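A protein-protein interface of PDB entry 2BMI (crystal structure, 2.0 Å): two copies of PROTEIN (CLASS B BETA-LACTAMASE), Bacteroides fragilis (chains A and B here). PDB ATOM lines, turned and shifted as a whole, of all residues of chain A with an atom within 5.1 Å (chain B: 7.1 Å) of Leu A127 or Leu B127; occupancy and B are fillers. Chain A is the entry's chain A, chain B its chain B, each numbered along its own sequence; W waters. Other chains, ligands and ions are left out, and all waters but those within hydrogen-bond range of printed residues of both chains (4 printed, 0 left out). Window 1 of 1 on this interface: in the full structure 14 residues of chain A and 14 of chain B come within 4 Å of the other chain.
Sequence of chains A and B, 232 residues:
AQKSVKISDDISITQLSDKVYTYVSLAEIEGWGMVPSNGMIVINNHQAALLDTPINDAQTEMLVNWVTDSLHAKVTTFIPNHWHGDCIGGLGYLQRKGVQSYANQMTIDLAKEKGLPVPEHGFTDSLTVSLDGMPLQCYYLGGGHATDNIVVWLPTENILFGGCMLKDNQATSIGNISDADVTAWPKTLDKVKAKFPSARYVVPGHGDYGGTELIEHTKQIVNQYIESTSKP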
ATOM      1  N   TYR A 102      -4.144   1.442  31.403  1.00  0.00           N
ATOM      2  CA  TYR A 102      -5.419   1.433  30.699  1.00  0.00           C
ATOM      3  C   TYR A 102      -5.701  -0.038  30.479  1.00  0.00           C
ATOM      4  O   TYR A 102      -4.791  -0.798  30.230  1.00  0.00           O
ATOM      5  CB  TYR A 102      -5.252   2.116  29.331  1.00  0.00           C
ATOM      6  CG  TYR A 102      -4.586   3.474  29.388  1.00  0.00           C
ATOM      7  CD1 TYR A 102      -3.198   3.590  29.561  1.00  0.00           C
ATOM      8  CD2 TYR A 102      -5.341   4.645  29.315  1.00  0.00           C
ATOM      9  CE1 TYR A 102      -2.584   4.835  29.672  1.00  0.00           C
ATOM     10  CE2 TYR A 102      -4.729   5.901  29.417  1.00  0.00           C
ATOM     11  CZ  TYR A 102      -3.355   5.981  29.598  1.00  0.00           C
ATOM     12  OH  TYR A 102      -2.745   7.204  29.712  1.00  0.00           O
ATOM     13  N   HIS A 121      -7.563   3.216  33.936  1.00  0.00           N
ATOM     14  CA  HIS A 121      -8.632   3.587  33.026  1.00  0.00           C
ATOM     15  C   HIS A 121      -9.183   2.400  32.278  1.00  0.00           C
ATOM     16  O   HIS A 121      -8.430   1.666  31.681  1.00  0.00           O
ATOM     17  CB  HIS A 121      -8.111   4.674  32.076  1.00  0.00           C
ATOM     18  CG  HIS A 121      -7.327   5.740  32.784  1.00  0.00           C
ATOM     19  ND1 HIS A 121      -7.880   6.553  33.747  1.00  0.00           N
ATOM     20  CD2 HIS A 121      -6.004   6.042  32.758  1.00  0.00           C
ATOM     21  CE1 HIS A 121      -6.931   7.293  34.299  1.00  0.00           C
ATOM     22  NE2 HIS A 121      -5.781   7.003  33.715  1.00  0.00           N
ATOM     23  N   GLY A 122     -10.505   2.230  32.303  1.00  0.00           N
ATOM     24  CA  GLY A 122     -11.102   1.104  31.613  1.00  0.00           C
ATOM     25  C   GLY A 122     -11.960   1.442  30.408  1.00  0.00           C
ATOM     26  O   GLY A 122     -12.771   2.350  30.460  1.00  0.00           O
ATOM     27  N   PHE A 123     -11.829   0.649  29.350  1.00  0.00           N
ATOM     28  CA  PHE A 123     -12.606   0.832  28.122  1.00  0.00           C
ATOM     29  C   PHE A 123     -13.450  -0.399  27.845  1.00  0.00           C
ATOM     30  O   PHE A 123     -13.129  -1.479  28.306  1.00  0.00           O
ATOM     31  CB  PHE A 123     -11.687   1.129  26.923  1.00  0.00           C
ATOM     32  CG  PHE A 123     -10.886  -0.044  26.447  1.00  0.00           C
ATOM     33  CD1 PHE A 123      -9.637  -0.303  26.976  1.00  0.00           C
ATOM     34  CD2 PHE A 123     -11.360  -0.860  25.427  1.00  0.00           C
ATOM     35  CE1 PHE A 123      -8.862  -1.359  26.487  1.00  0.00           C
ATOM     36  CE2 PHE A 123     -10.601  -1.908  24.936  1.00  0.00           C
ATOM     37  CZ  PHE A 123      -9.349  -2.160  25.466  1.00  0.00           C
ATOM     38  N   ASP A 125     -15.111  -0.996  24.330  1.00  0.00           N
ATOM     39  CA  ASP A 125     -15.074  -1.409  22.931  1.00  0.00           C
ATOM     40  C   ASP A 125     -13.646  -1.267  22.440  1.00  0.00           C
ATOM     41  O   ASP A 125     -12.964  -2.246  22.192  1.00  0.00           O
ATOM     42  CB  ASP A 125     -16.044  -0.525  22.119  1.00  0.00           C
ATOM     43  CG  ASP A 125     -16.026  -0.821  20.608  1.00  0.00           C
ATOM     44  OD1 ASP A 125     -15.426  -1.832  20.183  1.00  0.00           O
ATOM     45  OD2 ASP A 125     -16.617  -0.019  19.838  1.00  0.00           O
ATOM     46  N   SER A 126     -13.202  -0.035  22.259  1.00  0.00           N
ATOM     47  CA  SER A 126     -11.833   0.192  21.839  1.00  0.00           C
ATOM     48  C   SER A 126     -11.314   1.485  22.454  1.00  0.00           C
ATOM     49  O   SER A 126     -12.085   2.312  22.959  1.00  0.00           O
ATOM     50  CB  SER A 126     -11.704   0.183  20.308  1.00  0.00           C
ATOM     51  OG  SER A 126     -12.139   1.402  19.744  1.00  0.00           O
ATOM     52  N   LEU A 127      -9.996   1.601  22.489  1.00  0.00           N
ATOM     53  CA  LEU A 127      -9.333   2.755  23.044  1.00  0.00           C
ATOM     54  C   LEU A 127      -7.978   2.904  22.340  1.00  0.00           C
ATOM     55  O   LEU A 127      -7.243   1.919  22.165  1.00  0.00           O
ATOM     56  CB  LEU A 127      -9.099   2.556  24.546  1.00  0.00           C
ATOM     57  CG  LEU A 127      -8.280   3.630  25.248  1.00  0.00           C
ATOM     58  CD1 LEU A 127      -9.152   4.882  25.457  1.00  0.00           C
ATOM     59  CD2 LEU A 127      -7.792   3.086  26.584  1.00  0.00           C
ATOM     60  N   THR A 128      -7.670   4.124  21.903  1.00  0.00           N
ATOM     61  CA  THR A 128      -6.394   4.388  21.251  1.00  0.00           C
ATOM     62  C   THR A 128      -5.627   5.256  22.215  1.00  0.00           C
ATOM     63  O   THR A 128      -6.032   6.387  22.511  1.00  0.00           O
ATOM     64  CB  THR A 128      -6.553   5.140  19.904  1.00  0.00           C
ATOM     65  OG1 THR A 128      -7.389   4.377  19.025  1.00  0.00           O
ATOM     66  CG2 THR A 128      -5.186   5.361  19.238  1.00  0.00           C
ATOM     67  N   VAL A 129      -4.591   4.670  22.795  1.00  0.00           N
ATOM     68  CA  VAL A 129      -3.737   5.376  23.736  1.00  0.00           C
ATOM     69  C   VAL A 129      -2.615   6.045  22.955  1.00  0.00           C
ATOM     70  O   VAL A 129      -2.031   5.460  22.046  1.00  0.00           O
ATOM     71  CB  VAL A 129      -3.147   4.421  24.841  1.00  0.00           C
ATOM     72  CG1 VAL A 129      -2.119   5.186  25.731  1.00  0.00           C
ATOM     73  CG2 VAL A 129      -4.274   3.857  25.705  1.00  0.00           C
ATOM     74  N   LEU A 136      -1.618   3.525  20.122  1.00  0.00           N
ATOM     75  CA  LEU A 136      -1.654   2.172  20.704  1.00  0.00           C
ATOM     76  C   LEU A 136      -3.122   1.801  20.689  1.00  0.00           C
ATOM     77  O   LEU A 136      -3.860   2.176  21.594  1.00  0.00           O
ATOM     78  CB  LEU A 136      -1.165   2.215  22.163  1.00  0.00           C
ATOM     79  CG  LEU A 136       0.316   2.117  22.530  1.00  0.00           C
ATOM     80  CD1 LEU A 136       1.228   2.721  21.515  1.00  0.00           C
ATOM     81  CD2 LEU A 136       0.530   2.747  23.864  1.00  0.00           C
ATOM     82  N   GLN A 137      -3.560   1.076  19.668  1.00  0.00           N
ATOM     83  CA  GLN A 137      -4.978   0.726  19.559  1.00  0.00           C
ATOM     84  C   GLN A 137      -5.387  -0.578  20.236  1.00  0.00           C
ATOM     85  O   GLN A 137      -5.053  -1.664  19.781  1.00  0.00           O
ATOM     86  CB  GLN A 137      -5.418   0.716  18.092  1.00  0.00           C
ATOM     87  CG  GLN A 137      -5.030   1.969  17.320  1.00  0.00           C
ATOM     88  CD  GLN A 137      -5.618   2.011  15.919  1.00  0.00           C
ATOM     89  OE1 GLN A 137      -5.283   1.192  15.064  1.00  0.00           O
ATOM     90  NE2 GLN A 137      -6.503   2.972  15.681  1.00  0.00           N
ATOM     91  N   CYS A 138      -6.188  -0.433  21.279  1.00  0.00           N
ATOM     92  CA  CYS A 138      -6.680  -1.534  22.087  1.00  0.00           C
ATOM     93  C   CYS A 138      -8.100  -1.872  21.713  1.00  0.00           C
ATOM     94  O   CYS A 138      -8.964  -0.984  21.657  1.00  0.00           O
ATOM     95  CB  CYS A 138      -6.663  -1.133  23.567  1.00  0.00           C
ATOM     96  SG  CYS A 138      -5.122  -0.389  24.133  1.00  0.00           S
ATOM     97  N   ILE B  79     -11.576  16.314  29.746  1.00  0.00           N
ATOM     98  CA  ILE B  79     -12.470  15.594  28.852  1.00  0.00           C
ATOM     99  C   ILE B  79     -13.458  16.592  28.220  1.00  0.00           C
ATOM    100  O   ILE B  79     -14.186  17.277  28.939  1.00  0.00           O
ATOM    101  CB  ILE B  79     -13.322  14.559  29.606  1.00  0.00           C
ATOM    102  CG1 ILE B  79     -12.430  13.548  30.339  1.00  0.00           C
ATOM    103  CG2 ILE B  79     -14.237  13.836  28.602  1.00  0.00           C
ATOM    104  CD1 ILE B  79     -13.109  12.897  31.571  1.00  0.00           C
ATOM    105  N   SER B 101      -5.538  14.534  28.228  1.00  0.00           N
ATOM    106  CA  SER B 101      -6.915  14.540  27.731  1.00  0.00           C
ATOM    107  C   SER B 101      -7.425  13.244  27.106  1.00  0.00           C
ATOM    108  O   SER B 101      -6.675  12.461  26.523  1.00  0.00           O
ATOM    109  CB  SER B 101      -7.101  15.711  26.759  1.00  0.00           C
ATOM    110  OG  SER B 101      -6.020  15.758  25.851  1.00  0.00           O
ATOM    111  N   TYR B 102      -8.732  13.056  27.212  1.00  0.00           N
ATOM    112  CA  TYR B 102      -9.397  11.882  26.710  1.00  0.00           C
ATOM    113  C   TYR B 102     -10.662  12.406  26.071  1.00  0.00           C
ATOM    114  O   TYR B 102     -11.283  13.306  26.613  1.00  0.00           O
ATOM    115  CB  TYR B 102      -9.780  10.950  27.878  1.00  0.00           C
ATOM    116  CG  TYR B 102      -8.701  10.768  28.915  1.00  0.00           C
ATOM    117  CD1 TYR B 102      -8.400  11.787  29.822  1.00  0.00           C
ATOM    118  CD2 TYR B 102      -7.960   9.584  28.982  1.00  0.00           C
ATOM    119  CE1 TYR B 102      -7.385  11.641  30.768  1.00  0.00           C
ATOM    120  CE2 TYR B 102      -6.939   9.432  29.919  1.00  0.00           C
ATOM    121  CZ  TYR B 102      -6.659  10.465  30.804  1.00  0.00           C
ATOM    122  OH  TYR B 102      -5.629  10.348  31.711  1.00  0.00           O
ATOM    123  N   ALA B 103     -11.089  11.793  24.973  1.00  0.00           N
ATOM    124  CA  ALA B 103     -12.292  12.234  24.265  1.00  0.00           C
ATOM    125  C   ALA B 103     -12.758  11.140  23.341  1.00  0.00           C
ATOM    126  O   ALA B 103     -12.025  10.185  23.086  1.00  0.00           O
ATOM    127  CB  ALA B 103     -11.973  13.503  23.395  1.00  0.00           C
ATOM    128  N   ASN B 104     -13.951  11.329  22.788  1.00  0.00           N
ATOM    129  CA  ASN B 104     -14.533  10.410  21.818  1.00  0.00           C
ATOM    130  C   ASN B 104     -13.547  10.416  20.651  1.00  0.00           C
ATOM    131  O   ASN B 104     -13.065  11.483  20.272  1.00  0.00           O
ATOM    132  CB  ASN B 104     -15.872  10.993  21.365  1.00  0.00           C
ATOM    133  CG  ASN B 104     -16.593  10.135  20.341  1.00  0.00           C
ATOM    134  OD1 ASN B 104     -16.040   9.190  19.795  1.00  0.00           O
ATOM    135  ND2 ASN B 104     -17.841  10.487  20.062  1.00  0.00           N
ATOM    136  N   GLN B 105     -13.197   9.252  20.105  1.00  0.00           N
ATOM    137  CA  GLN B 105     -12.264   9.239  18.986  1.00  0.00           C
ATOM    138  C   GLN B 105     -12.773  10.120  17.853  1.00  0.00           C
ATOM    139  O   GLN B 105     -11.978  10.659  17.072  1.00  0.00           O
ATOM    140  CB  GLN B 105     -12.014   7.836  18.473  1.00  0.00           C
ATOM    141  CG  GLN B 105     -10.974   7.787  17.343  1.00  0.00           C
ATOM    142  CD  GLN B 105      -9.562   8.200  17.773  1.00  0.00           C
ATOM    143  OE1 GLN B 105      -9.100   7.870  18.866  1.00  0.00           O
ATOM    144  NE2 GLN B 105      -8.879   8.931  16.910  1.00  0.00           N
ATOM    145  N   HIS B 121      -6.132  10.848  24.113  1.00  0.00           N
ATOM    146  CA  HIS B 121      -6.626   9.476  24.042  1.00  0.00           C
ATOM    147  C   HIS B 121      -8.053   9.397  23.584  1.00  0.00           C
ATOM    148  O   HIS B 121      -8.909  10.088  24.114  1.00  0.00           O
ATOM    149  CB  HIS B 121      -6.448   8.822  25.411  1.00  0.00           C
ATOM    150  CG  HIS B 121      -5.125   9.149  26.052  1.00  0.00           C
ATOM    151  ND1 HIS B 121      -3.922   8.825  25.466  1.00  0.00           N
ATOM    152  CD2 HIS B 121      -4.825   9.851  27.176  1.00  0.00           C
ATOM    153  CE1 HIS B 121      -2.937   9.333  26.194  1.00  0.00           C
ATOM    154  NE2 HIS B 121      -3.456   9.956  27.235  1.00  0.00           N
ATOM    155  N   GLY B 122      -8.314   8.542  22.596  1.00  0.00           N
ATOM    156  CA  GLY B 122      -9.668   8.436  22.084  1.00  0.00           C
ATOM    157  C   GLY B 122     -10.355   7.118  22.352  1.00  0.00           C
ATOM    158  O   GLY B 122      -9.713   6.086  22.293  1.00  0.00           O
ATOM    159  N   PHE B 123     -11.642   7.162  22.679  1.00  0.00           N
ATOM    160  CA  PHE B 123     -12.434   5.955  22.915  1.00  0.00           C
ATOM    161  C   PHE B 123     -13.571   5.897  21.912  1.00  0.00           C
ATOM    162  O   PHE B 123     -13.928   6.920  21.341  1.00  0.00           O
ATOM    163  CB  PHE B 123     -12.996   5.931  24.338  1.00  0.00           C
ATOM    164  CG  PHE B 123     -14.077   6.949  24.614  1.00  0.00           C
ATOM    165  CD1 PHE B 123     -15.420   6.629  24.430  1.00  0.00           C
ATOM    166  CD2 PHE B 123     -13.764   8.184  25.180  1.00  0.00           C
ATOM    167  CE1 PHE B 123     -16.428   7.519  24.814  1.00  0.00           C
ATOM    168  CE2 PHE B 123     -14.762   9.066  25.565  1.00  0.00           C
ATOM    169  CZ  PHE B 123     -16.095   8.731  25.386  1.00  0.00           C
ATOM    170  N   THR B 124     -14.155   4.722  21.695  1.00  0.00           N
ATOM    171  CA  THR B 124     -15.263   4.621  20.763  1.00  0.00           C
ATOM    172  C   THR B 124     -16.633   4.374  21.376  1.00  0.00           C
ATOM    173  O   THR B 124     -17.656   4.824  20.840  1.00  0.00           O
ATOM    174  CB  THR B 124     -15.019   3.547  19.755  1.00  0.00           C
ATOM    175  OG1 THR B 124     -14.733   2.329  20.440  1.00  0.00           O
ATOM    176  CG2 THR B 124     -13.844   3.915  18.876  1.00  0.00           C
ATOM    177  N   ASP B 125     -16.675   3.694  22.509  1.00  0.00           N
ATOM    178  CA  ASP B 125     -17.954   3.385  23.136  1.00  0.00           C
ATOM    179  C   ASP B 125     -18.028   4.031  24.508  1.00  0.00           C
ATOM    180  O   ASP B 125     -18.795   4.961  24.738  1.00  0.00           O
ATOM    181  CB  ASP B 125     -18.095   1.859  23.258  1.00  0.00           C
ATOM    182  CG  ASP B 125     -19.320   1.436  24.034  1.00  0.00           C
ATOM    183  OD1 ASP B 125     -20.337   2.152  24.007  1.00  0.00           O
ATOM    184  OD2 ASP B 125     -19.275   0.364  24.671  1.00  0.00           O
ATOM    185  N   SER B 126     -17.253   3.502  25.439  1.00  0.00           N
ATOM    186  CA  SER B 126     -17.246   4.055  26.765  1.00  0.00           C
ATOM    187  C   SER B 126     -15.840   4.048  27.291  1.00  0.00           C
ATOM    188  O   SER B 126     -14.975   3.332  26.783  1.00  0.00           O
ATOM    189  CB  SER B 126     -18.139   3.249  27.676  1.00  0.00           C
ATOM    190  OG  SER B 126     -18.029   3.777  28.979  1.00  0.00           O
ATOM    191  N   LEU B 127     -15.587   4.912  28.265  1.00  0.00           N
ATOM    192  CA  LEU B 127     -14.273   4.994  28.892  1.00  0.00           C
ATOM    193  C   LEU B 127     -14.437   5.592  30.278  1.00  0.00           C
ATOM    194  O   LEU B 127     -15.001   6.675  30.446  1.00  0.00           O
ATOM    195  CB  LEU B 127     -13.296   5.856  28.070  1.00  0.00           C
ATOM    196  CG  LEU B 127     -11.950   6.227  28.722  1.00  0.00           C
ATOM    197  CD1 LEU B 127     -11.061   4.984  28.849  1.00  0.00           C
ATOM    198  CD2 LEU B 127     -11.241   7.298  27.898  1.00  0.00           C
ATOM    199  N   THR B 128     -14.016   4.832  31.280  1.00  0.00           N
ATOM    200  CA  THR B 128     -14.072   5.306  32.643  1.00  0.00           C
ATOM    201  C   THR B 128     -12.685   5.820  32.980  1.00  0.00           C
ATOM    202  O   THR B 128     -11.732   5.059  33.033  1.00  0.00           O
ATOM    203  CB  THR B 128     -14.511   4.196  33.594  1.00  0.00           C
ATOM    204  OG1 THR B 128     -15.808   3.749  33.181  1.00  0.00           O
ATOM    205  CG2 THR B 128     -14.611   4.717  35.020  1.00  0.00           C
ATOM    206  N   VAL B 129     -12.563   7.134  33.097  1.00  0.00           N
ATOM    207  CA  VAL B 129     -11.289   7.753  33.428  1.00  0.00           C
ATOM    208  C   VAL B 129     -11.244   7.786  34.950  1.00  0.00           C
ATOM    209  O   VAL B 129     -12.217   8.197  35.588  1.00  0.00           O
ATOM    210  CB  VAL B 129     -11.201   9.184  32.831  1.00  0.00           C
ATOM    211  CG1 VAL B 129      -9.963   9.893  33.327  1.00  0.00           C
ATOM    212  CG2 VAL B 129     -11.218   9.116  31.317  1.00  0.00           C
ATOM    213  N   SER B 130     -10.165   7.262  35.531  1.00  0.00           N
ATOM    214  CA  SER B 130     -10.018   7.223  36.978  1.00  0.00           C
ATOM    215  C   SER B 130      -9.279   8.449  37.519  1.00  0.00           C
ATOM    216  O   SER B 130      -8.084   8.602  37.272  1.00  0.00           O
ATOM    217  CB  SER B 130      -9.257   5.966  37.387  1.00  0.00           C
ATOM    218  OG  SER B 130      -9.085   5.949  38.787  1.00  0.00           O
ATOM    219  N   LEU B 136     -14.932   8.657  36.327  1.00  0.00           N
ATOM    220  CA  LEU B 136     -15.535   9.668  35.457  1.00  0.00           C
ATOM    221  C   LEU B 136     -15.885   8.840  34.213  1.00  0.00           C
ATOM    222  O   LEU B 136     -15.035   8.594  33.354  1.00  0.00           O
ATOM    223  CB  LEU B 136     -14.504  10.742  35.099  1.00  0.00           C
ATOM    224  CG  LEU B 136     -13.639  11.373  36.199  1.00  0.00           C
ATOM    225  CD1 LEU B 136     -12.656  12.333  35.557  1.00  0.00           C
ATOM    226  CD2 LEU B 136     -14.455  12.066  37.236  1.00  0.00           C
ATOM    227  N   GLN B 137     -17.128   8.387  34.149  1.00  0.00           N
ATOM    228  CA  GLN B 137     -17.583   7.514  33.073  1.00  0.00           C
ATOM    229  C   GLN B 137     -18.097   8.234  31.845  1.00  0.00           C
ATOM    230  O   GLN B 137     -19.192   8.813  31.863  1.00  0.00           O
ATOM    231  CB  GLN B 137     -18.650   6.564  33.614  1.00  0.00           C
ATOM    232  CG  GLN B 137     -18.208   5.810  34.875  1.00  0.00           C
ATOM    233  CD  GLN B 137     -19.214   4.771  35.323  1.00  0.00           C
ATOM    234  OE1 GLN B 137     -20.364   5.090  35.632  1.00  0.00           O
ATOM    235  NE2 GLN B 137     -18.781   3.515  35.374  1.00  0.00           N
ATOM    236  N   CYS B 138     -17.298   8.160  30.783  1.00  0.00           N
ATOM    237  CA  CYS B 138     -17.573   8.789  29.486  1.00  0.00           C
ATOM    238  C   CYS B 138     -18.255   7.821  28.533  1.00  0.00           C
ATOM    239  O   CYS B 138     -17.761   6.720  28.310  1.00  0.00           O
ATOM    240  CB  CYS B 138     -16.256   9.255  28.858  1.00  0.00           C
ATOM    241  SG  CYS B 138     -15.245  10.276  29.949  1.00  0.00           S
ATOM    242  N   TYR B 139     -19.381   8.235  27.958  1.00  0.00           N
ATOM    243  CA  TYR B 139     -20.125   7.392  27.023  1.00  0.00           C
ATOM    244  C   TYR B 139     -20.490   8.073  25.720  1.00  0.00           C
ATOM    245  O   TYR B 139     -20.930   9.214  25.725  1.00  0.00           O
ATOM    246  CB  TYR B 139     -21.477   6.954  27.623  1.00  0.00           C
ATOM    247  CG  TYR B 139     -21.402   6.171  28.903  1.00  0.00           C
ATOM    248  CD1 TYR B 139     -21.310   4.771  28.888  1.00  0.00           C
ATOM    249  CD2 TYR B 139     -21.435   6.828  30.137  1.00  0.00           C
ATOM    250  CE1 TYR B 139     -21.253   4.048  30.084  1.00  0.00           C
ATOM    251  CE2 TYR B 139     -21.375   6.120  31.334  1.00  0.00           C
ATOM    252  CZ  TYR B 139     -21.279   4.733  31.305  1.00  0.00           C
ATOM    253  OH  TYR B 139     -21.170   4.043  32.493  1.00  0.00           O
ATOM    254  N   TYR B 140     -20.302   7.379  24.607  1.00  0.00           N
ATOM    255  CA  TYR B 140     -20.752   7.902  23.325  1.00  0.00           C
ATOM    256  C   TYR B 140     -22.001   7.063  23.021  1.00  0.00           C
ATOM    257  O   TYR B 140     -21.914   5.838  22.870  1.00  0.00           O
ATOM    258  CB  TYR B 140     -19.737   7.730  22.212  1.00  0.00           C
ATOM    259  CG  TYR B 140     -20.325   8.181  20.895  1.00  0.00           C
ATOM    260  CD1 TYR B 140     -20.794   9.493  20.725  1.00  0.00           C
ATOM    261  CD2 TYR B 140     -20.477   7.286  19.845  1.00  0.00           C
ATOM    262  CE1 TYR B 140     -21.389   9.887  19.543  1.00  0.00           C
ATOM    263  CE2 TYR B 140     -21.079   7.672  18.662  1.00  0.00           C
ATOM    264  CZ  TYR B 140     -21.528   8.968  18.519  1.00  0.00           C
ATOM    265  OH  TYR B 140     -22.106   9.321  17.331  1.00  0.00           O
ATOM    266  N   VAL B 151     -21.452  12.013  26.813  1.00  0.00           N
ATOM    267  CA  VAL B 151     -21.969  12.442  28.105  1.00  0.00           C
ATOM    268  C   VAL B 151     -20.949  11.909  29.108  1.00  0.00           C
ATOM    269  O   VAL B 151     -20.237  10.932  28.825  1.00  0.00           O
ATOM    270  CB  VAL B 151     -23.394  11.875  28.480  1.00  0.00           C
ATOM    271  CG1 VAL B 151     -24.434  12.264  27.443  1.00  0.00           C
ATOM    272  CG2 VAL B 151     -23.353  10.361  28.718  1.00  0.00           C
HETATM  273  O   HOH W   1     -10.076   4.994  19.472  1.00  0.00           O
HETATM  274  O   HOH W   2     -15.783   1.999  31.167  1.00  0.00           O
HETATM  275  O   HOH W   3     -14.221   2.107  24.264  1.00  0.00           O
HETATM  276  O   HOH W   4      -3.742   8.687  31.452  1.00  0.00           O
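Among the printed residues, merely in contact across the chains: Asp A125 with Asp B125 (3.3 Å), Gly A122 with Leu B127 (3.4 Å), Leu A127 with Gly B122 (3.4 Å), His A121 with Thr B128 (3.4 Å), Thr A128 with His B121 (3.5 Å), His A121 with Val B129 (3.6 Å), Ser A126 with Phe B123 (3.7 Å), Phe A123 with Ser B126 (3.7 Å), Tyr A102 with His B121 (3.8 Å), Val A129 with His B121 (3.9 Å), Thr A128 with Gln B105 (3.9 Å), Leu A127 with Leu B127 (3.9 Å) and His A121 with Tyr B102 (3.9 Å).
Hydrophobic or aromatic side chains of chain A that line the printed part of chain B: Tyr A102, His A121, Phe A123 and Leu A127. Along chain A the printed residues that touch a printed residue of chain B span positions 102 to 129. Of the 22 printed residues of chain B, 12 touch a printed residue of chain A.
O of Val A129 is in hydrogen-bond range of N of Leu A136, 2.8 Å away. O of Ser B101 lies within hydrogen-bond range of N of His B121, at 3.0 Å. The backbone NH of Ala B103 sits at hydrogen-bond distance from the backbone carbonyl oxygen of His B121 (2.9 Å). The backbone carbonyl oxygen (O) of Cys B138 is in hydrogen-bond range of the side-chain hydroxyl (OG) of Ser B126, 3.0 Å away. O of Leu B127 sits at hydrogen-bond distance from N of Cys B138, at 2.8 Å. O of Val B129 is in hydrogen-bond range of N of Leu B136 (2.9 Å).
Of chain B, only Gly B122 and Leu B127 come within 4 Å of Leu A127. Of the printed residues of chain A, Thr B124 touches Asp A125 and Ser A126. Of the printed residues of chain A, Asp B125 touches Asp A125 (3.3 Å). Printed residues of chain A within 4 Å of Tyr B102: His A121.
A ring nitrogen (ND1) of His A121 is in hydrogen-bond range of the backbone NH (N) of Ser B130, 3.0 Å away. N of Thr B128 is in hydrogen-bond range of O of Gly A122 (2.9 Å). The side-chain hydroxyl (OG1) of Thr B124 lies within hydrogen-bond range of the side-chain carboxylate (OD2) of Asp A125 (3.1 Å). OG of Ser A126 sits at hydrogen-bond distance from OG1 of Thr B124, at 2.8 Å. The backbone carbonyl oxygen (O) of Gly B122 is in hydrogen-bond range of the backbone NH (N) of Thr A128, at 2.9 Å.
Tyr A102 touches His B121, and with the chains exchanged His A121 touches Tyr B102. Gly A122 touches Leu B127, and with the chains exchanged Leu A127 touches Gly B122. Gly A122 touches Thr B128, and with the chains exchanged Thr A128 touches Gly B122. Asp B125 touches its own counterpart, Asp A125. 12 positions are printed for both chains. Of the 18 pairs that touch across the chains among the printed residues, 14 have their exchanged pair printed and touching as well.
Water W4 lies within hydrogen-bond range of the side-chain hydroxyl of Tyr A102 (2.5 Å), the side-chain hydroxyl of Tyr B102 (2.5 Å) and a ring nitrogen (NE2) of His A121 (3.5 Å). Water W3 lies within hydrogen-bond range of the backbone carbonyl oxygen of Ser A126 (2.5 Å), the backbone carbonyl oxygen of Ser B126 (2.9 Å), the backbone NH of Asp A125 (3.2 Å) and the backbone NH of Asp B125 (3.4 Å). Water W2 lies within hydrogen-bond range of the side-chain hydroxyl of Thr B128 (2.7 Å) and the backbone carbonyl oxygen of Gly A122 (3.1 Å). Water W1 lies within hydrogen-bond range of OG1 of Thr A128 (2.8 Å), O of Gly B122 (3.0 Å) and OE1 of Gln B105 (3.1 Å).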
